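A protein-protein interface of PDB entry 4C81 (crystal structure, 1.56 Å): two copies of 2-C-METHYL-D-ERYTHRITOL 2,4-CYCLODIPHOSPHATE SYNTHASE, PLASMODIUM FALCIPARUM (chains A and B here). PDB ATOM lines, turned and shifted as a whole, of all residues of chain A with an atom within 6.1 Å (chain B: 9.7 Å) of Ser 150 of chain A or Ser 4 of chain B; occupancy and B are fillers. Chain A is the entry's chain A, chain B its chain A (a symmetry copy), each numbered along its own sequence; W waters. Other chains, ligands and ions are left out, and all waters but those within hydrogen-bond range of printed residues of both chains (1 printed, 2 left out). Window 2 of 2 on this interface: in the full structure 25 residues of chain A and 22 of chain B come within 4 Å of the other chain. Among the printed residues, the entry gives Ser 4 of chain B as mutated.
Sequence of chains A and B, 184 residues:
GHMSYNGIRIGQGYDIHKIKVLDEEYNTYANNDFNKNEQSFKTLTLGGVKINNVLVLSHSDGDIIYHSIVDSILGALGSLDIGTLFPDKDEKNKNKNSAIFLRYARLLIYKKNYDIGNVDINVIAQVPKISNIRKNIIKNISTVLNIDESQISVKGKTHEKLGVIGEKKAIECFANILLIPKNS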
ATOM      1  N   ASN A 118     -29.955  -4.860 -22.691  1.00  0.00           N
ATOM      2  CA  ASN A 118     -30.307  -5.910 -21.741  1.00  0.00           C
ATOM      3  C   ASN A 118     -31.762  -5.785 -21.314  1.00  0.00           C
ATOM      4  O   ASN A 118     -32.403  -4.765 -21.561  1.00  0.00           O
ATOM      5  CB  ASN A 118     -29.393  -5.877 -20.517  1.00  0.00           C
ATOM      6  CG  ASN A 118     -29.716  -4.734 -19.583  1.00  0.00           C
ATOM      7  OD1 ASN A 118     -29.730  -3.575 -19.991  1.00  0.00           O
ATOM      8  ND2 ASN A 118     -29.998  -5.056 -18.328  1.00  0.00           N
ATOM      9  N   ILE A 138     -34.408 -18.100 -18.850  1.00  0.00           N
ATOM     10  CA  ILE A 138     -33.362 -17.323 -19.516  1.00  0.00           C
ATOM     11  C   ILE A 138     -32.971 -17.948 -20.861  1.00  0.00           C
ATOM     12  O   ILE A 138     -32.764 -17.230 -21.846  1.00  0.00           O
ATOM     13  CB  ILE A 138     -32.127 -17.136 -18.601  1.00  0.00           C
ATOM     14  CG1 ILE A 138     -32.473 -16.191 -17.443  1.00  0.00           C
ATOM     15  CG2 ILE A 138     -30.947 -16.589 -19.387  1.00  0.00           C
ATOM     16  CD1 ILE A 138     -31.361 -16.016 -16.434  1.00  0.00           C
ATOM     17  N   ASP A 148     -28.007 -13.064 -26.313  1.00  0.00           N
ATOM     18  CA  ASP A 148     -27.173 -13.854 -25.418  1.00  0.00           C
ATOM     19  C   ASP A 148     -27.784 -13.872 -24.022  1.00  0.00           C
ATOM     20  O   ASP A 148     -28.427 -12.906 -23.608  1.00  0.00           O
ATOM     21  CB  ASP A 148     -25.761 -13.272 -25.360  1.00  0.00           C
ATOM     22  CG  ASP A 148     -24.767 -14.220 -24.722  1.00  0.00           C
ATOM     23  OD1 ASP A 148     -24.454 -15.258 -25.342  1.00  0.00           O
ATOM     24  OD2 ASP A 148     -24.309 -13.935 -23.595  1.00  0.00           O
ATOM     25  N   GLU A 149     -27.569 -14.969 -23.299  1.00  0.00           N
ATOM     26  CA  GLU A 149     -28.096 -15.126 -21.942  1.00  0.00           C
ATOM     27  C   GLU A 149     -27.556 -14.071 -20.974  1.00  0.00           C
ATOM     28  O   GLU A 149     -28.215 -13.739 -19.984  1.00  0.00           O
ATOM     29  CB  GLU A 149     -27.791 -16.530 -21.405  1.00  0.00           C
ATOM     30  CG  GLU A 149     -28.497 -17.647 -22.169  1.00  0.00           C
ATOM     31  CD  GLU A 149     -28.229 -19.025 -21.590  1.00  0.00           C
ATOM     32  OE1 GLU A 149     -27.357 -19.154 -20.704  1.00  0.00           O
ATOM     33  OE2 GLU A 149     -28.895 -19.986 -22.025  1.00  0.00           O
ATOM     34  N   SER A 150     -26.369 -13.539 -21.270  1.00  0.00           N
ATOM     35  CA  SER A 150     -25.768 -12.474 -20.464  1.00  0.00           C
ATOM     36  C   SER A 150     -26.517 -11.139 -20.554  1.00  0.00           C
ATOM     37  O   SER A 150     -26.242 -10.223 -19.775  1.00  0.00           O
ATOM     38  CB  SER A 150     -24.305 -12.257 -20.869  1.00  0.00           C
ATOM     39  OG  SER A 150     -24.209 -11.661 -22.152  1.00  0.00           O
ATOM     40  N   GLN A 151     -27.443 -11.025 -21.506  1.00  0.00           N
ATOM     41  CA  GLN A 151     -28.275  -9.829 -21.654  1.00  0.00           C
ATOM     42  C   GLN A 151     -29.620  -9.936 -20.929  1.00  0.00           C
ATOM     43  O   GLN A 151     -30.451  -9.036 -21.059  1.00  0.00           O
ATOM     44  CB  GLN A 151     -28.531  -9.553 -23.137  1.00  0.00           C
ATOM     45  CG  GLN A 151     -27.275  -9.216 -23.919  1.00  0.00           C
ATOM     46  CD  GLN A 151     -27.494  -9.227 -25.419  1.00  0.00           C
ATOM     47  OE1 GLN A 151     -27.173 -10.205 -26.091  1.00  0.00           O
ATOM     48  NE2 GLN A 151     -28.044  -8.145 -25.949  1.00  0.00           N
ATOM     49  N   ILE A 152     -29.831 -11.021 -20.181  1.00  0.00           N
ATOM     50  CA  ILE A 152     -31.128 -11.308 -19.550  1.00  0.00           C
ATOM     51  C   ILE A 152     -31.001 -11.535 -18.040  1.00  0.00           C
ATOM     52  O   ILE A 152     -30.131 -12.276 -17.581  1.00  0.00           O
ATOM     53  CB  ILE A 152     -31.777 -12.566 -20.165  1.00  0.00           C
ATOM     54  CG1 ILE A 152     -31.891 -12.430 -21.687  1.00  0.00           C
ATOM     55  CG2 ILE A 152     -33.152 -12.818 -19.553  1.00  0.00           C
ATOM     56  CD1 ILE A 152     -32.269 -13.723 -22.378  1.00  0.00           C
ATOM     57  N   SER B   4     -19.723 -11.457 -24.292  1.00  0.00           N
ATOM     58  CA  SER B   4     -20.904 -10.987 -23.512  1.00  0.00           C
ATOM     59  C   SER B   4     -21.201  -9.515 -23.793  1.00  0.00           C
ATOM     60  O   SER B   4     -20.384  -8.809 -24.388  1.00  0.00           O
ATOM     61  CB  SER B   4     -20.670 -11.200 -22.015  1.00  0.00           C
ATOM     62  OG  SER B   4     -19.511 -10.513 -21.576  1.00  0.00           O
ATOM     63  N   TYR B   5     -22.374  -9.061 -23.358  1.00  0.00           N
ATOM     64  CA  TYR B   5     -22.801  -7.678 -23.575  1.00  0.00           C
ATOM     65  C   TYR B   5     -22.106  -6.743 -22.592  1.00  0.00           C
ATOM     66  O   TYR B   5     -22.184  -6.938 -21.375  1.00  0.00           O
ATOM     67  CB  TYR B   5     -24.325  -7.566 -23.447  1.00  0.00           C
ATOM     68  CG  TYR B   5     -24.868  -6.155 -23.574  1.00  0.00           C
ATOM     69  CD1 TYR B   5     -24.860  -5.490 -24.797  1.00  0.00           C
ATOM     70  CD2 TYR B   5     -25.391  -5.488 -22.464  1.00  0.00           C
ATOM     71  CE1 TYR B   5     -25.357  -4.190 -24.913  1.00  0.00           C
ATOM     72  CE2 TYR B   5     -25.888  -4.196 -22.569  1.00  0.00           C
ATOM     73  CZ  TYR B   5     -25.874  -3.547 -23.793  1.00  0.00           C
ATOM     74  OH  TYR B   5     -26.361  -2.265 -23.914  1.00  0.00           O
ATOM     75  N   ASN B   6     -21.419  -5.734 -23.127  1.00  0.00           N
ATOM     76  CA  ASN B   6     -20.667  -4.776 -22.318  1.00  0.00           C
ATOM     77  C   ASN B   6     -21.133  -3.335 -22.544  1.00  0.00           C
ATOM     78  O   ASN B   6     -20.374  -2.390 -22.318  1.00  0.00           O
ATOM     79  CB  ASN B   6     -19.163  -4.902 -22.617  1.00  0.00           C
ATOM     80  CG  ASN B   6     -18.525  -6.122 -21.956  1.00  0.00           C
ATOM     81  OD1 ASN B   6     -19.210  -7.012 -21.452  1.00  0.00           O
ATOM     82  ND2 ASN B   6     -17.198  -6.159 -21.959  1.00  0.00           N
ATOM     83  N   GLY B   7     -22.382  -3.170 -22.976  1.00  0.00           N
ATOM     84  CA  GLY B   7     -22.954  -1.844 -23.199  1.00  0.00           C
ATOM     85  C   GLY B   7     -23.734  -1.354 -21.994  1.00  0.00           C
ATOM     86  O   GLY B   7     -23.704  -1.976 -20.930  1.00  0.00           O
ATOM     87  N   ILE B   8     -24.439  -0.238 -22.169  1.00  0.00           N
ATOM     88  CA  ILE B   8     -25.246   0.334 -21.095  1.00  0.00           C
ATOM     89  C   ILE B   8     -26.289  -0.685 -20.624  1.00  0.00           C
ATOM     90  O   ILE B   8     -26.890  -1.391 -21.435  1.00  0.00           O
ATOM     91  CB  ILE B   8     -25.916   1.666 -21.534  1.00  0.00           C
ATOM     92  CG1 ILE B   8     -26.582   2.358 -20.340  1.00  0.00           C
ATOM     93  CG2 ILE B   8     -26.922   1.431 -22.656  1.00  0.00           C
ATOM     94  CD1 ILE B   8     -27.063   3.759 -20.648  1.00  0.00           C
ATOM     95  N   ARG B   9     -26.481  -0.759 -19.308  1.00  0.00           N
ATOM     96  CA  ARG B   9     -27.392  -1.731 -18.696  1.00  0.00           C
ATOM     97  C   ARG B   9     -28.414  -1.050 -17.796  1.00  0.00           C
ATOM     98  O   ARG B   9     -28.078  -0.142 -17.034  1.00  0.00           O
ATOM     99  CB  ARG B   9     -26.606  -2.763 -17.884  1.00  0.00           C
ATOM    100  CG  ARG B   9     -25.947  -3.839 -18.741  1.00  0.00           C
ATOM    101  CD  ARG B   9     -24.952  -4.668 -17.950  1.00  0.00           C
ATOM    102  NE  ARG B   9     -24.407  -5.765 -18.752  1.00  0.00           N
ATOM    103  CZ  ARG B   9     -24.982  -6.956 -18.927  1.00  0.00           C
ATOM    104  NH1 ARG B   9     -26.149  -7.255 -18.355  1.00  0.00           N
ATOM    105  NH2 ARG B   9     -24.381  -7.868 -19.684  1.00  0.00           N
ATOM    106  N   ILE B  10     -29.660  -1.507 -17.909  1.00  0.00           N
ATOM    107  CA  ILE B  10     -30.766  -1.067 -17.062  1.00  0.00           C
ATOM    108  C   ILE B  10     -31.059  -2.129 -16.007  1.00  0.00           C
ATOM    109  O   ILE B  10     -31.009  -3.334 -16.280  1.00  0.00           O
ATOM    110  CB  ILE B  10     -32.055  -0.798 -17.900  1.00  0.00           C
ATOM    111  CG1 ILE B  10     -33.169  -0.189 -17.037  1.00  0.00           C
ATOM    112  CG2 ILE B  10     -32.555  -2.075 -18.558  1.00  0.00           C
ATOM    113  CD1 ILE B  10     -34.344   0.316 -17.844  1.00  0.00           C
ATOM    114  N   LEU B  74     -27.777  -6.120  -9.341  1.00  0.00           N
ATOM    115  CA  LEU B  74     -27.670  -7.520  -9.749  1.00  0.00           C
ATOM    116  C   LEU B  74     -28.484  -7.757 -11.016  1.00  0.00           C
ATOM    117  O   LEU B  74     -28.015  -8.396 -11.959  1.00  0.00           O
ATOM    118  CB  LEU B  74     -28.154  -8.451  -8.635  1.00  0.00           C
ATOM    119  CG  LEU B  74     -27.270  -8.486  -7.389  1.00  0.00           C
ATOM    120  CD1 LEU B  74     -27.872  -9.385  -6.321  1.00  0.00           C
ATOM    121  CD2 LEU B  74     -25.873  -8.947  -7.760  1.00  0.00           C
ATOM    122  N   GLY B  75     -29.702  -7.225 -11.034  1.00  0.00           N
ATOM    123  CA  GLY B  75     -30.577  -7.359 -12.190  1.00  0.00           C
ATOM    124  C   GLY B  75     -29.966  -6.773 -13.452  1.00  0.00           C
ATOM    125  O   GLY B  75     -30.003  -7.386 -14.521  1.00  0.00           O
ATOM    126  N   ALA B  76     -29.386  -5.585 -13.323  1.00  0.00           N
ATOM    127  CA  ALA B  76     -28.739  -4.911 -14.446  1.00  0.00           C
ATOM    128  C   ALA B  76     -27.610  -5.746 -15.055  1.00  0.00           C
ATOM    129  O   ALA B  76     -27.446  -5.766 -16.276  1.00  0.00           O
ATOM    130  CB  ALA B  76     -28.203  -3.557 -14.007  1.00  0.00           C
ATOM    131  N   LEU B  77     -26.855  -6.433 -14.202  1.00  0.00           N
ATOM    132  CA  LEU B  77     -25.688  -7.204 -14.632  1.00  0.00           C
ATOM    133  C   LEU B  77     -26.009  -8.660 -14.984  1.00  0.00           C
ATOM    134  O   LEU B  77     -25.136  -9.394 -15.452  1.00  0.00           O
ATOM    135  CB  LEU B  77     -24.609  -7.157 -13.545  1.00  0.00           C
ATOM    136  CG  LEU B  77     -23.991  -5.776 -13.326  1.00  0.00           C
ATOM    137  CD1 LEU B  77     -23.243  -5.707 -11.998  1.00  0.00           C
ATOM    138  CD2 LEU B  77     -23.077  -5.400 -14.487  1.00  0.00           C
ATOM    139  N   GLY B  78     -27.254  -9.078 -14.767  1.00  0.00           N
ATOM    140  CA  GLY B  78     -27.650 -10.456 -15.036  1.00  0.00           C
ATOM    141  C   GLY B  78     -27.192 -11.451 -13.986  1.00  0.00           C
ATOM    142  O   GLY B  78     -27.170 -12.656 -14.242  1.00  0.00           O
ATOM    143  N   SER B  79     -26.802 -10.954 -12.813  1.00  0.00           N
ATOM    144  CA  SER B  79     -26.365 -11.818 -11.725  1.00  0.00           C
ATOM    145  C   SER B  79     -27.583 -12.415 -11.038  1.00  0.00           C
ATOM    146  O   SER B  79     -28.697 -11.916 -11.192  1.00  0.00           O
ATOM    147  CB  SER B  79     -25.529 -11.035 -10.710  1.00  0.00           C
ATOM    148  OG  SER B  79     -24.336 -10.538 -11.292  1.00  0.00           O
ATOM    149  N   LYS B 112     -16.854  -5.937 -12.952  1.00  0.00           N
ATOM    150  CA  LYS B 112     -17.432  -6.091 -14.293  1.00  0.00           C
ATOM    151  C   LYS B 112     -17.140  -4.887 -15.203  1.00  0.00           C
ATOM    152  O   LYS B 112     -17.662  -4.812 -16.320  1.00  0.00           O
ATOM    153  CB  LYS B 112     -18.944  -6.334 -14.193  1.00  0.00           C
ATOM    154  CG  LYS B 112     -19.326  -7.617 -13.454  1.00  0.00           C
ATOM    155  CD  LYS B 112     -19.079  -8.874 -14.286  1.00  0.00           C
ATOM    156  CE  LYS B 112     -20.189  -9.128 -15.295  1.00  0.00           C
ATOM    157  NZ  LYS B 112     -21.469  -9.512 -14.639  1.00  0.00           N
ATOM    158  N   TYR B 114     -17.905  -1.607 -14.813  1.00  0.00           N
ATOM    159  CA  TYR B 114     -19.017  -0.665 -14.944  1.00  0.00           C
ATOM    160  C   TYR B 114     -18.910   0.447 -13.895  1.00  0.00           C
ATOM    161  O   TYR B 114     -18.262   0.279 -12.859  1.00  0.00           O
ATOM    162  CB  TYR B 114     -20.365  -1.392 -14.799  1.00  0.00           C
ATOM    163  CG  TYR B 114     -20.875  -2.013 -16.079  1.00  0.00           C
ATOM    164  CD1 TYR B 114     -21.623  -1.268 -16.985  1.00  0.00           C
ATOM    165  CD2 TYR B 114     -20.622  -3.346 -16.380  1.00  0.00           C
ATOM    166  CE1 TYR B 114     -22.092  -1.824 -18.163  1.00  0.00           C
ATOM    167  CE2 TYR B 114     -21.083  -3.917 -17.557  1.00  0.00           C
ATOM    168  CZ  TYR B 114     -21.820  -3.151 -18.445  1.00  0.00           C
ATOM    169  OH  TYR B 114     -22.285  -3.713 -19.608  1.00  0.00           O
HETATM  170  O   HOH W   1     -30.074  -7.771 -17.277  1.00  0.00           O
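The backbone NH of Tyr 5 of chain B lies within hydrogen-bond range of the side-chain hydroxyl of Ser 150 of chain A (3.4 Å). ND2 of Asn 118 of chain A lies within hydrogen-bond range of O of Ala 76 of chain B. The backbone carbonyl oxygen (O) of Ser 150 of chain A sits at hydrogen-bond distance from the guanidinium group (NH2) of Arg 9 of chain B. The side-chain amide nitrogen (ND2) of Asn 118 of chain A sits at hydrogen-bond distance from the backbone carbonyl oxygen (O) of Ile 10 of chain B (2.9 Å).
The side-chain amide oxygen of Gln 151 of chain A lies within hydrogen-bond range of the backbone NH of Asp 148 of chain A, at 3.0 Å. The side-chain carboxylate of Asp 148 of chain A is in hydrogen-bond range of the side-chain hydroxyl of Ser 150 of chain A (2.7 Å). The guanidinium group of Arg 9 of chain B lies within hydrogen-bond range of the backbone carbonyl oxygen of Ala 76 of chain B. The backbone carbonyl oxygen of Tyr 5 of chain B sits at hydrogen-bond distance from the guanidinium group of Arg 9 of chain B, 2.9 Å away. OH of Tyr 114 of chain B lies within hydrogen-bond range of NE of Arg 9 of chain B. The backbone carbonyl oxygen of Ile 8 of chain B lies within hydrogen-bond range of the side-chain hydroxyl of Tyr 5 of chain B (2.7 Å).
Among the printed residues, merely in contact across the chains: Asn 118 of chain A with Arg 9 of chain B (3.2 Å), Gln 151 of chain A with Tyr 5 of chain B (3.4 Å), Ser 150 of chain A with Ser 4 of chain B (3.6 Å), Asn 118 of chain A with Ile 8 of chain B (3.9 Å) and Ile 152 of chain A with Gly 78 of chain B (3.99 Å).
Of the printed residues of chain B, Asn 118 of chain A touches Ile 8 (3.9 Å), Arg 9 (3.2 Å), Ile 10 (2.9 Å) and Ala 76 (3.4 Å). No residue of chain B comes within 4 Å of Asp 148 of chain A. Of chain B, only Ser 4, Tyr 5 and Arg 9 come within 4 Å of Ser 150 of chain A. Of the printed residues of chain A, Tyr 5 of chain B touches Ser 150 and Gln 151. Of the printed residues of chain A, Ile 8 of chain B touches Asn 118 (3.9 Å). Of the printed residues of chain A, Arg 9 of chain B touches Asn 118 (3.2 Å) and Ser 150 (3.0 Å). Of the printed residues of chain A, Ile 10 of chain B touches Asn 118 (2.9 Å). Leu 74 of chain B touches none of the printed residues of chain A. Ser 79 of chain B touches none of the printed residues of chain A. The nearest residue of chain A that does not touch Ser 4 of chain B is Asp 148 of chain A (4.5 Å).
Of the 15 printed residues of chain B, 7 touch a printed residue of chain A. Printed residues of chain B that touch a printed residue of chain A: Ser 4, Tyr 5, Ile 8, Arg 9, Ile 10, Ala 76 and Gly 78. Of the 7 printed residues of chain A, 4 touch a printed residue of chain B. Printed residues of chain A that touch a printed residue of chain B: Asn 118, Ser 150, Gln 151 and Ile 152.
No position is printed for both chains. Of the 9 pairs that touch across the chains among the printed residues, none has its exchanged pair printed and touching as well.
Water W1 lies within hydrogen-bond range of O of Gly 75 of chain B (2.8 Å), ND2 of Asn 118 of chain A (2.9 Å) and O of Ala 76 of chain B (3.5 Å).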
